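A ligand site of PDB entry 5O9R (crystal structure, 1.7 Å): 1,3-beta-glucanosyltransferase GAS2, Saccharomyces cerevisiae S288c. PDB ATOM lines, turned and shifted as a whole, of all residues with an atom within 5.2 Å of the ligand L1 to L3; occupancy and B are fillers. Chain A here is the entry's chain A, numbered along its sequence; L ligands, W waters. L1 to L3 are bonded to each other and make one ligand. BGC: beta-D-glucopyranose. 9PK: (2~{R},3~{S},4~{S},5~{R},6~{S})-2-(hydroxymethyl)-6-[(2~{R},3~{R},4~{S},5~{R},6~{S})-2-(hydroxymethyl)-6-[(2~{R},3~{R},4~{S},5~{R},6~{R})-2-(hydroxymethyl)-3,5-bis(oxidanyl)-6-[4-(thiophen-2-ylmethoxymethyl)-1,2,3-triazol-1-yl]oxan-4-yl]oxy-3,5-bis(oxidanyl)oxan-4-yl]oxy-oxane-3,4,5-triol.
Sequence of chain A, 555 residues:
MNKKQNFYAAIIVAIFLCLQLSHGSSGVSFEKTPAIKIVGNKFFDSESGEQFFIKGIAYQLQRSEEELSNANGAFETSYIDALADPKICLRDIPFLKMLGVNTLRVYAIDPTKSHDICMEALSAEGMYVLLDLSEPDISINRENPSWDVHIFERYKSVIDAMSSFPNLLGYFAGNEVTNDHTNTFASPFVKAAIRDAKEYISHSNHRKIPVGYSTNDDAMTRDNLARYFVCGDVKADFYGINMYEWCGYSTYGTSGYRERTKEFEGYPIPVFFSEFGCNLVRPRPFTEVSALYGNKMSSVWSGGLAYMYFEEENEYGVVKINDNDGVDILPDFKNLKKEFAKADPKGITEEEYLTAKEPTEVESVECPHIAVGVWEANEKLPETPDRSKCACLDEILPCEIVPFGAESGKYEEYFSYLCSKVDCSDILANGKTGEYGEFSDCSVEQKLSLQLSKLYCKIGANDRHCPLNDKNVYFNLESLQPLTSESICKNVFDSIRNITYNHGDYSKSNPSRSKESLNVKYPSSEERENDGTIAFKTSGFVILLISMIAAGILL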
ATOM      1  N   ASN A 179       8.453  -0.778  19.290  1.00  0.00           N
ATOM      2  CA  ASN A 179       8.003  -0.105  18.050  1.00  0.00           C
ATOM      3  C   ASN A 179       8.699   1.208  17.705  1.00  0.00           C
ATOM      4  O   ASN A 179       8.439   1.773  16.637  1.00  0.00           O
ATOM      5  CB  ASN A 179       6.473   0.052  18.040  1.00  0.00           C
ATOM      6  CG  ASN A 179       5.943   0.917  19.170  1.00  0.00           C
ATOM      7  OD1 ASN A 179       6.690   1.569  19.913  1.00  0.00           O
ATOM      8  ND2 ASN A 179       4.610   0.934  19.315  1.00  0.00           N
ATOM      9  N   ASN A 216       7.148  -3.969  13.334  1.00  0.00           N
ATOM     10  CA  ASN A 216       6.704  -2.813  12.536  1.00  0.00           C
ATOM     11  C   ASN A 216       7.824  -2.361  11.573  1.00  0.00           C
ATOM     12  O   ASN A 216       8.703  -3.154  11.246  1.00  0.00           O
ATOM     13  CB  ASN A 216       6.165  -1.704  13.456  1.00  0.00           C
ATOM     14  CG  ASN A 216       7.250  -1.048  14.300  1.00  0.00           C
ATOM     15  OD1 ASN A 216       8.220  -1.691  14.669  1.00  0.00           O
ATOM     16  ND2 ASN A 216       7.051   0.224  14.623  1.00  0.00           N
ATOM     17  N   ASP A 217       7.786  -1.108  11.105  1.00  0.00           N
ATOM     18  CA  ASP A 217       8.711  -0.638  10.074  1.00  0.00           C
ATOM     19  C   ASP A 217       9.265   0.759  10.387  1.00  0.00           C
ATOM     20  O   ASP A 217       9.403   1.609   9.492  1.00  0.00           O
ATOM     21  CB  ASP A 217       7.983  -0.655   8.720  1.00  0.00           C
ATOM     22  CG  ASP A 217       8.907  -0.462   7.539  1.00  0.00           C
ATOM     23  OD1 ASP A 217      10.082  -0.879   7.599  1.00  0.00           O
ATOM     24  OD2 ASP A 217       8.454   0.124   6.542  1.00  0.00           O
ATOM     25  N   ASP A 218       9.606   0.979  11.659  1.00  0.00           N
ATOM     26  CA  ASP A 218      10.195   2.249  12.106  1.00  0.00           C
ATOM     27  C   ASP A 218      11.632   2.330  11.605  1.00  0.00           C
ATOM     28  O   ASP A 218      12.432   1.416  11.817  1.00  0.00           O
ATOM     29  CB  ASP A 218      10.127   2.344  13.632  1.00  0.00           C
ATOM     30  CG  ASP A 218      10.856   3.547  14.191  1.00  0.00           C
ATOM     31  OD1 ASP A 218      10.319   4.663  14.084  1.00  0.00           O
ATOM     32  OD2 ASP A 218      11.951   3.352  14.764  1.00  0.00           O
ATOM     33  N   ALA A 219      11.971   3.429  10.911  1.00  0.00           N
ATOM     34  CA  ALA A 219      13.270   3.559  10.250  1.00  0.00           C
ATOM     35  C   ALA A 219      14.455   3.504  11.209  1.00  0.00           C
ATOM     36  O   ALA A 219      15.486   2.924  10.866  1.00  0.00           O
ATOM     37  CB  ALA A 219      13.314   4.859   9.445  1.00  0.00           C
ATOM     38  N   ARG A 222      14.487  -0.569  12.716  1.00  0.00           N
ATOM     39  CA  ARG A 222      14.235  -1.810  11.937  1.00  0.00           C
ATOM     40  C   ARG A 222      15.463  -2.685  11.688  1.00  0.00           C
ATOM     41  O   ARG A 222      15.369  -3.906  11.809  1.00  0.00           O
ATOM     42  CB  ARG A 222      13.518  -1.514  10.624  1.00  0.00           C
ATOM     43  CG  ARG A 222      14.281  -0.655   9.635  1.00  0.00           C
ATOM     44  CD  ARG A 222      13.360  -0.302   8.474  1.00  0.00           C
ATOM     45  NE  ARG A 222      13.903   0.761   7.640  1.00  0.00           N
ATOM     46  CZ  ARG A 222      13.205   1.429   6.724  1.00  0.00           C
ATOM     47  NH1 ARG A 222      11.919   1.139   6.505  1.00  0.00           N
ATOM     48  NH2 ARG A 222      13.790   2.393   6.023  1.00  0.00           N
ATOM     49  N   ASN A 242       5.427  -5.876   9.225  1.00  0.00           N
ATOM     50  CA  ASN A 242       4.179  -5.215   8.866  1.00  0.00           C
ATOM     51  C   ASN A 242       4.554  -4.033   7.978  1.00  0.00           C
ATOM     52  O   ASN A 242       5.060  -3.027   8.454  1.00  0.00           O
ATOM     53  CB  ASN A 242       3.407  -4.822  10.130  1.00  0.00           C
ATOM     54  CG  ASN A 242       3.049  -6.033  10.980  1.00  0.00           C
ATOM     55  OD1 ASN A 242       2.769  -7.107  10.457  1.00  0.00           O
ATOM     56  ND2 ASN A 242       3.059  -5.871  12.298  1.00  0.00           N
ATOM     57  N   TYR A 244       4.018  -1.259   5.076  1.00  0.00           N
ATOM     58  CA  TYR A 244       3.064  -0.330   4.448  1.00  0.00           C
ATOM     59  C   TYR A 244       3.728   0.744   3.563  1.00  0.00           C
ATOM     60  O   TYR A 244       3.138   1.781   3.294  1.00  0.00           O
ATOM     61  CB  TYR A 244       2.200   0.313   5.532  1.00  0.00           C
ATOM     62  CG  TYR A 244       1.293  -0.676   6.229  1.00  0.00           C
ATOM     63  CD1 TYR A 244       0.000  -0.905   5.756  1.00  0.00           C
ATOM     64  CD2 TYR A 244       1.726  -1.393   7.335  1.00  0.00           C
ATOM     65  CE1 TYR A 244      -0.843  -1.814   6.373  1.00  0.00           C
ATOM     66  CE2 TYR A 244       0.884  -2.305   7.966  1.00  0.00           C
ATOM     67  CZ  TYR A 244      -0.395  -2.514   7.474  1.00  0.00           C
ATOM     68  OH  TYR A 244      -1.242  -3.414   8.086  1.00  0.00           O
ATOM     69  N   GLU A 245       4.940   0.462   3.098  1.00  0.00           N
ATOM     70  CA  GLU A 245       5.716   1.434   2.312  1.00  0.00           C
ATOM     71  C   GLU A 245       5.145   1.715   0.911  1.00  0.00           C
ATOM     72  O   GLU A 245       5.335   2.805   0.386  1.00  0.00           O
ATOM     73  CB  GLU A 245       7.176   1.002   2.186  1.00  0.00           C
ATOM     74  CG  GLU A 245       7.949   1.113   3.494  1.00  0.00           C
ATOM     75  CD  GLU A 245       9.358   0.558   3.392  1.00  0.00           C
ATOM     76  OE1 GLU A 245       9.914   0.471   2.278  1.00  0.00           O
ATOM     77  OE2 GLU A 245       9.933   0.216   4.441  1.00  0.00           O
ATOM     78  N   CYS A 247       2.274   2.617  -1.322  1.00  0.00           N
ATOM     79  CA  CYS A 247       0.932   3.209  -1.347  1.00  0.00           C
ATOM     80  C   CYS A 247       0.535   3.547  -2.783  1.00  0.00           C
ATOM     81  O   CYS A 247       1.332   4.133  -3.528  1.00  0.00           O
ATOM     82  CB  CYS A 247       0.883   4.460  -0.478  1.00  0.00           C
ATOM     83  SG  CYS A 247       1.313   4.182   1.262  1.00  0.00           S
ATOM     84  N   THR A 254      10.792   3.171  -6.048  1.00  0.00           N
ATOM     85  CA  THR A 254      10.315   4.355  -5.311  1.00  0.00           C
ATOM     86  C   THR A 254       9.621   4.042  -3.987  1.00  0.00           C
ATOM     87  O   THR A 254       9.628   4.883  -3.077  1.00  0.00           O
ATOM     88  CB  THR A 254       9.380   5.224  -6.181  1.00  0.00           C
ATOM     89  OG1 THR A 254       8.216   4.477  -6.559  1.00  0.00           O
ATOM     90  CG2 THR A 254      10.103   5.697  -7.438  1.00  0.00           C
ATOM     91  N   SER A 255       9.015   2.864  -3.870  1.00  0.00           N
ATOM     92  CA  SER A 255       8.315   2.460  -2.641  1.00  0.00           C
ATOM     93  C   SER A 255       9.254   2.293  -1.443  1.00  0.00           C
ATOM     94  O   SER A 255       8.873   2.588  -0.312  1.00  0.00           O
ATOM     95  CB  SER A 255       7.544   1.151  -2.844  1.00  0.00           C
ATOM     96  OG  SER A 255       8.426   0.079  -3.167  1.00  0.00           O
ATOM     97  N   ARG A 260      14.619  -2.469   0.980  1.00  0.00           N
ATOM     98  CA  ARG A 260      14.273  -3.517   1.972  1.00  0.00           C
ATOM     99  C   ARG A 260      14.773  -4.887   1.522  1.00  0.00           C
ATOM    100  O   ARG A 260      15.306  -5.660   2.314  1.00  0.00           O
ATOM    101  CB  ARG A 260      12.752  -3.606   2.207  1.00  0.00           C
ATOM    102  CG  ARG A 260      12.085  -2.360   2.762  1.00  0.00           C
ATOM    103  CD  ARG A 260      12.570  -1.969   4.152  1.00  0.00           C
ATOM    104  NE  ARG A 260      13.785  -1.149   4.136  1.00  0.00           N
ATOM    105  CZ  ARG A 260      13.867   0.126   3.716  1.00  0.00           C
ATOM    106  NH1 ARG A 260      12.797   0.777   3.254  1.00  0.00           N
ATOM    107  NH2 ARG A 260      15.029   0.751   3.772  1.00  0.00           N
ATOM    108  N   CYS A 278      -1.159  -0.603   2.256  1.00  0.00           N
ATOM    109  CA  CYS A 278      -1.357   0.833   2.495  1.00  0.00           C
ATOM    110  C   CYS A 278      -2.618   1.288   1.772  1.00  0.00           C
ATOM    111  O   CYS A 278      -2.806   0.975   0.583  1.00  0.00           O
ATOM    112  CB  CYS A 278      -0.164   1.633   1.993  1.00  0.00           C
ATOM    113  SG  CYS A 278      -0.372   3.418   2.108  1.00  0.00           S
ATOM    114  N   LEU A 280      -3.763   4.578   1.459  1.00  0.00           N
ATOM    115  CA  LEU A 280      -3.720   5.994   1.107  1.00  0.00           C
ATOM    116  C   LEU A 280      -4.568   6.276  -0.135  1.00  0.00           C
ATOM    117  O   LEU A 280      -5.393   7.195  -0.124  1.00  0.00           O
ATOM    118  CB  LEU A 280      -2.276   6.442   0.850  1.00  0.00           C
ATOM    119  CG  LEU A 280      -1.989   7.905   0.513  1.00  0.00           C
ATOM    120  CD1 LEU A 280      -2.412   8.823   1.648  1.00  0.00           C
ATOM    121  CD2 LEU A 280      -0.518   8.101   0.184  1.00  0.00           C
HETATM  122  C2  BGC L   1       7.089   5.964   1.919  1.00  0.00           C
HETATM  123  C3  BGC L   1       5.845   5.344   2.557  1.00  0.00           C
HETATM  124  C4  BGC L   1       4.765   6.421   2.537  1.00  0.00           C
HETATM  125  C5  BGC L   1       4.394   6.644   1.064  1.00  0.00           C
HETATM  126  C6  BGC L   1       3.305   7.688   0.884  1.00  0.00           C
HETATM  127  C1  BGC L   1       6.724   6.174   0.442  1.00  0.00           C
HETATM  128  O1  BGC L   1       7.829   6.744  -0.271  1.00  0.00           O
HETATM  129  O2  BGC L   1       8.258   5.151   2.004  1.00  0.00           O
HETATM  130  O3  BGC L   1       5.976   4.594   3.785  1.00  0.00           O
HETATM  131  O4  BGC L   1       3.615   6.048   3.310  1.00  0.00           O
HETATM  132  O5  BGC L   1       5.569   7.030   0.315  1.00  0.00           O
HETATM  133  O6  BGC L   1       3.001   7.855  -0.506  1.00  0.00           O
HETATM  134  C2  BGC L   2       6.369   4.049   6.024  1.00  0.00           C
HETATM  135  C3  BGC L   2       7.295   4.018   7.242  1.00  0.00           C
HETATM  136  C4  BGC L   2       8.715   3.768   6.777  1.00  0.00           C
HETATM  137  C5  BGC L   2       9.104   4.825   5.748  1.00  0.00           C
HETATM  138  C6  BGC L   2      10.569   4.751   5.323  1.00  0.00           C
HETATM  139  C1  BGC L   2       6.870   4.936   4.871  1.00  0.00           C
HETATM  140  O2  BGC L   2       5.068   4.468   6.450  1.00  0.00           O
HETATM  141  O3  BGC L   2       6.882   2.957   8.126  1.00  0.00           O
HETATM  142  O4  BGC L   2       9.610   3.743   7.889  1.00  0.00           O
HETATM  143  O5  BGC L   2       8.248   4.682   4.606  1.00  0.00           O
HETATM  144  O6  BGC L   2      10.877   3.573   4.577  1.00  0.00           O
HETATM  145  C2  BGC L   3       5.762   2.223  10.107  1.00  0.00           C
HETATM  146  C3  BGC L   3       5.202   2.628  11.476  1.00  0.00           C
HETATM  147  C4  BGC L   3       6.135   3.580  12.214  1.00  0.00           C
HETATM  148  C5  BGC L   3       6.555   4.739  11.316  1.00  0.00           C
HETATM  149  C6  BGC L   3       7.559   5.642  12.008  1.00  0.00           C
HETATM  150  C1  BGC L   3       6.249   3.438   9.329  1.00  0.00           C
HETATM  151  O2  BGC L   3       4.772   1.500   9.350  1.00  0.00           O
HETATM  152  O3  BGC L   3       5.025   1.440  12.253  1.00  0.00           O
HETATM  153  O4  BGC L   3       5.478   4.067  13.383  1.00  0.00           O
HETATM  154  O5  BGC L   3       7.137   4.203  10.126  1.00  0.00           O
HETATM  155  O6  BGC L   3       7.972   6.660  11.099  1.00  0.00           O
HETATM  156  C4  9PK L   4      -1.693  -8.192  20.614  1.00  0.00           C
HETATM  157  C5  9PK L   4      -1.710  -8.411  19.114  1.00  0.00           C
HETATM  158  C6  9PK L   4      -1.767  -9.912  18.819  1.00  0.00           C
HETATM  159  C3  9PK L   4      -1.642  -6.700  20.900  1.00  0.00           C
HETATM  160  CBT 9PK L   4      -0.994   2.401  10.534  1.00  0.00           C
HETATM  161  CBS 9PK L   4       0.124   3.157  10.625  1.00  0.00           C
HETATM  162  CBR 9PK L   4       1.239   2.575  10.181  1.00  0.00           C
HETATM  163  SBQ 9PK L   4       0.813   1.053   9.644  1.00  0.00           S
HETATM  164  CBP 9PK L   4      -0.759   1.190  10.004  1.00  0.00           C
HETATM  165  CBN 9PK L   4      -1.821   0.110   9.770  1.00  0.00           C
HETATM  166  OBO 9PK L   4      -1.852  -0.774  10.889  1.00  0.00           O
HETATM  167  CBM 9PK L   4      -2.801  -1.810  10.643  1.00  0.00           C
HETATM  168  CBL 9PK L   4      -3.211  -2.448  11.975  1.00  0.00           C
HETATM  169  CBH 9PK L   4      -3.125  -3.735  12.278  1.00  0.00           C
HETATM  170  NBK 9PK L   4      -3.702  -1.810  13.024  1.00  0.00           N
HETATM  171  NBJ 9PK L   4      -3.915  -2.643  13.899  1.00  0.00           N
HETATM  172  NBI 9PK L   4      -3.593  -3.795  13.517  1.00  0.00           N
HETATM  173  CAG 9PK L   4      -3.712  -5.036  14.328  1.00  0.00           C
HETATM  174  CAK 9PK L   4      -3.632  -4.717  15.818  1.00  0.00           C
HETATM  175  OBA 9PK L   4      -2.386  -4.081  16.104  1.00  0.00           O
HETATM  176  OAY 9PK L   4      -4.967  -5.676  14.041  1.00  0.00           O
HETATM  177  CAI 9PK L   4      -5.007  -6.947  14.693  1.00  0.00           C
HETATM  178  CAJ 9PK L   4      -6.282  -7.691  14.280  1.00  0.00           C
HETATM  179  OBB 9PK L   4      -7.387  -6.790  14.284  1.00  0.00           O
HETATM  180  CAH 9PK L   4      -5.013  -6.748  16.196  1.00  0.00           C
HETATM  181  OAZ 9PK L   4      -5.049  -8.027  16.853  1.00  0.00           O
HETATM  182  CAL 9PK L   4      -3.749  -6.003  16.617  1.00  0.00           C
HETATM  183  O1  9PK L   4      -3.814  -5.698  18.013  1.00  0.00           O
HETATM  184  C1  9PK L   4      -2.733  -6.350  18.700  1.00  0.00           C
HETATM  185  C2  9PK L   4      -2.782  -5.994  20.179  1.00  0.00           C
HETATM  186  O2  9PK L   4      -2.652  -4.579  20.331  1.00  0.00           O
HETATM  187  O5  9PK L   4      -2.860  -7.769  18.539  1.00  0.00           O
HETATM  188  O6  9PK L   4      -2.889 -10.492  19.509  1.00  0.00           O
HETATM  189  O4  9PK L   4      -0.547  -8.827  21.183  1.00  0.00           O
HETATM  190  O3  9PK L   4      -1.769  -6.473  22.317  1.00  0.00           O
HETATM  191  CAM 9PK L   4      -0.839  -5.459  22.720  1.00  0.00           C
HETATM  192  OBD 9PK L   4       0.502  -5.915  22.523  1.00  0.00           O
HETATM  193  CAO 9PK L   4       1.423  -4.849  22.816  1.00  0.00           C
HETATM  194  CAP 9PK L   4       2.850  -5.305  22.482  1.00  0.00           C
HETATM  195  OBG 9PK L   4       3.076  -6.608  23.033  1.00  0.00           O
HETATM  196  CAN 9PK L   4       1.344  -4.499  24.289  1.00  0.00           C
HETATM  197  OBE 9PK L   4       2.252  -3.431  24.575  1.00  0.00           O
HETATM  198  CAR 9PK L   4      -0.079  -4.052  24.627  1.00  0.00           C
HETATM  199  OBC 9PK L   4      -0.194  -3.849  26.037  1.00  0.00           O
HETATM  200  CAQ 9PK L   4      -1.054  -5.130  24.197  1.00  0.00           C
HETATM  201  OBF 9PK L   4      -2.403  -4.658  24.383  1.00  0.00           O
HETATM  202  O   HOH W   1       2.666   1.045  13.298  1.00  0.00           O
HETATM  203  O   HOH W   2      10.111   5.483   9.920  1.00  0.00           O
HETATM  204  O   HOH W   3       2.905   4.125   4.849  1.00  0.00           O
HETATM  205  O   HOH W   4      10.363   3.631   1.993  1.00  0.00           O
HETATM  206  O   HOH W   5       5.601   0.588   6.507  1.00  0.00           O
HETATM  207  O   HOH W   6       7.124   4.029  15.452  1.00  0.00           O
HETATM  208  O   HOH W   7       4.758  -1.026  10.316  1.00  0.00           O
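Water W3 lies within hydrogen-bond range of an oxygen (O4) of BGC L1 (2.6 Å) and the backbone carbonyl oxygen of Tyr 244 (2.8 Å).
Water W4 lies within hydrogen-bond range of an oxygen (O2) of BGC L1 (2.6 Å), the backbone carbonyl oxygen of Ser 255 (2.9 Å) and the side-chain carboxylate of Glu 245 (3.2 Å).
Water W6 bridges O4 of BGC L3 and O of Asn 179.
Water W7 lies within hydrogen-bond range of an oxygen (O2) of BGC L3, the backbone carbonyl oxygen of Asn 242 and the backbone NH of Asp 217.
Water W2 bridges an oxygen (O6) of BGC L3 (2.7 Å) and the backbone NH of Ala 219 (2.9 Å).
Water W5 lies within hydrogen-bond range of N of Tyr 244, OD2 of Asp 217, O2 of BGC L3 and N of Glu 245.
The side-chain carboxylate of Asp 217 lies within salt-bridge range of the guanidinium group of Arg 222 (2.9 Å).
The side-chain carboxylate of Asp 217 sits close to the side-chain carboxylate of Glu 245, 2.6 Å away.
The side-chain carboxylate of Glu 245 is in salt-bridge range of the guanidinium group of Arg 222 (3.0 Å).
The side-chain amide nitrogen (ND2) of Asn 216 is in hydrogen-bond range of the backbone carbonyl oxygen (O) of Asn 179.
The side-chain carboxylate (OE1) of Glu 245 is in salt-bridge range of the guanidinium group (NH1) of Arg 260.
The side-chain sulfur (SG) of Cys 278 sits close to the backbone NH (N) of Leu 280 (3.6 Å).
SG of Cys 247 is disulfide-bonded to SG of Cys 278 (2.0 Å).
An oxygen (O4) of BGC L2 lies within hydrogen-bond range of the backbone carbonyl oxygen (O) of Asp 217 (2.7 Å).
The guanidinium group (NH1) of Arg 222 is in hydrogen-bond range of an oxygen (O6) of BGC L2 (3.3 Å).
The side-chain amide nitrogen of Asn 216 sits at hydrogen-bond distance from an oxygen (O3) of BGC L3 (3.3 Å).
An oxygen (O6) of BGC L2 sits at hydrogen-bond distance from the side-chain carboxylate (OE2) of Glu 245, 3.5 Å away.
SG of Cys 247 is in hydrogen-bond range of O4 of BGC L1 (3.6 Å).
Asp 218 touches the ligand L1 to L3.
N of Ala 219 touches O4 of BGC L2 (3.8 Å).
Thr 254 touches the ligand L1 to L3.
O of Ser 255 touches O2 of BGC L1, at 3.5 Å.
Arg 260 touches the ligand L1 to L3.
CD2 of Leu 280 touches O6 of BGC L1, at 3.6 Å.
Hydrophobic or aromatic side chains that line the ligand L1 to L3: Leu 280.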
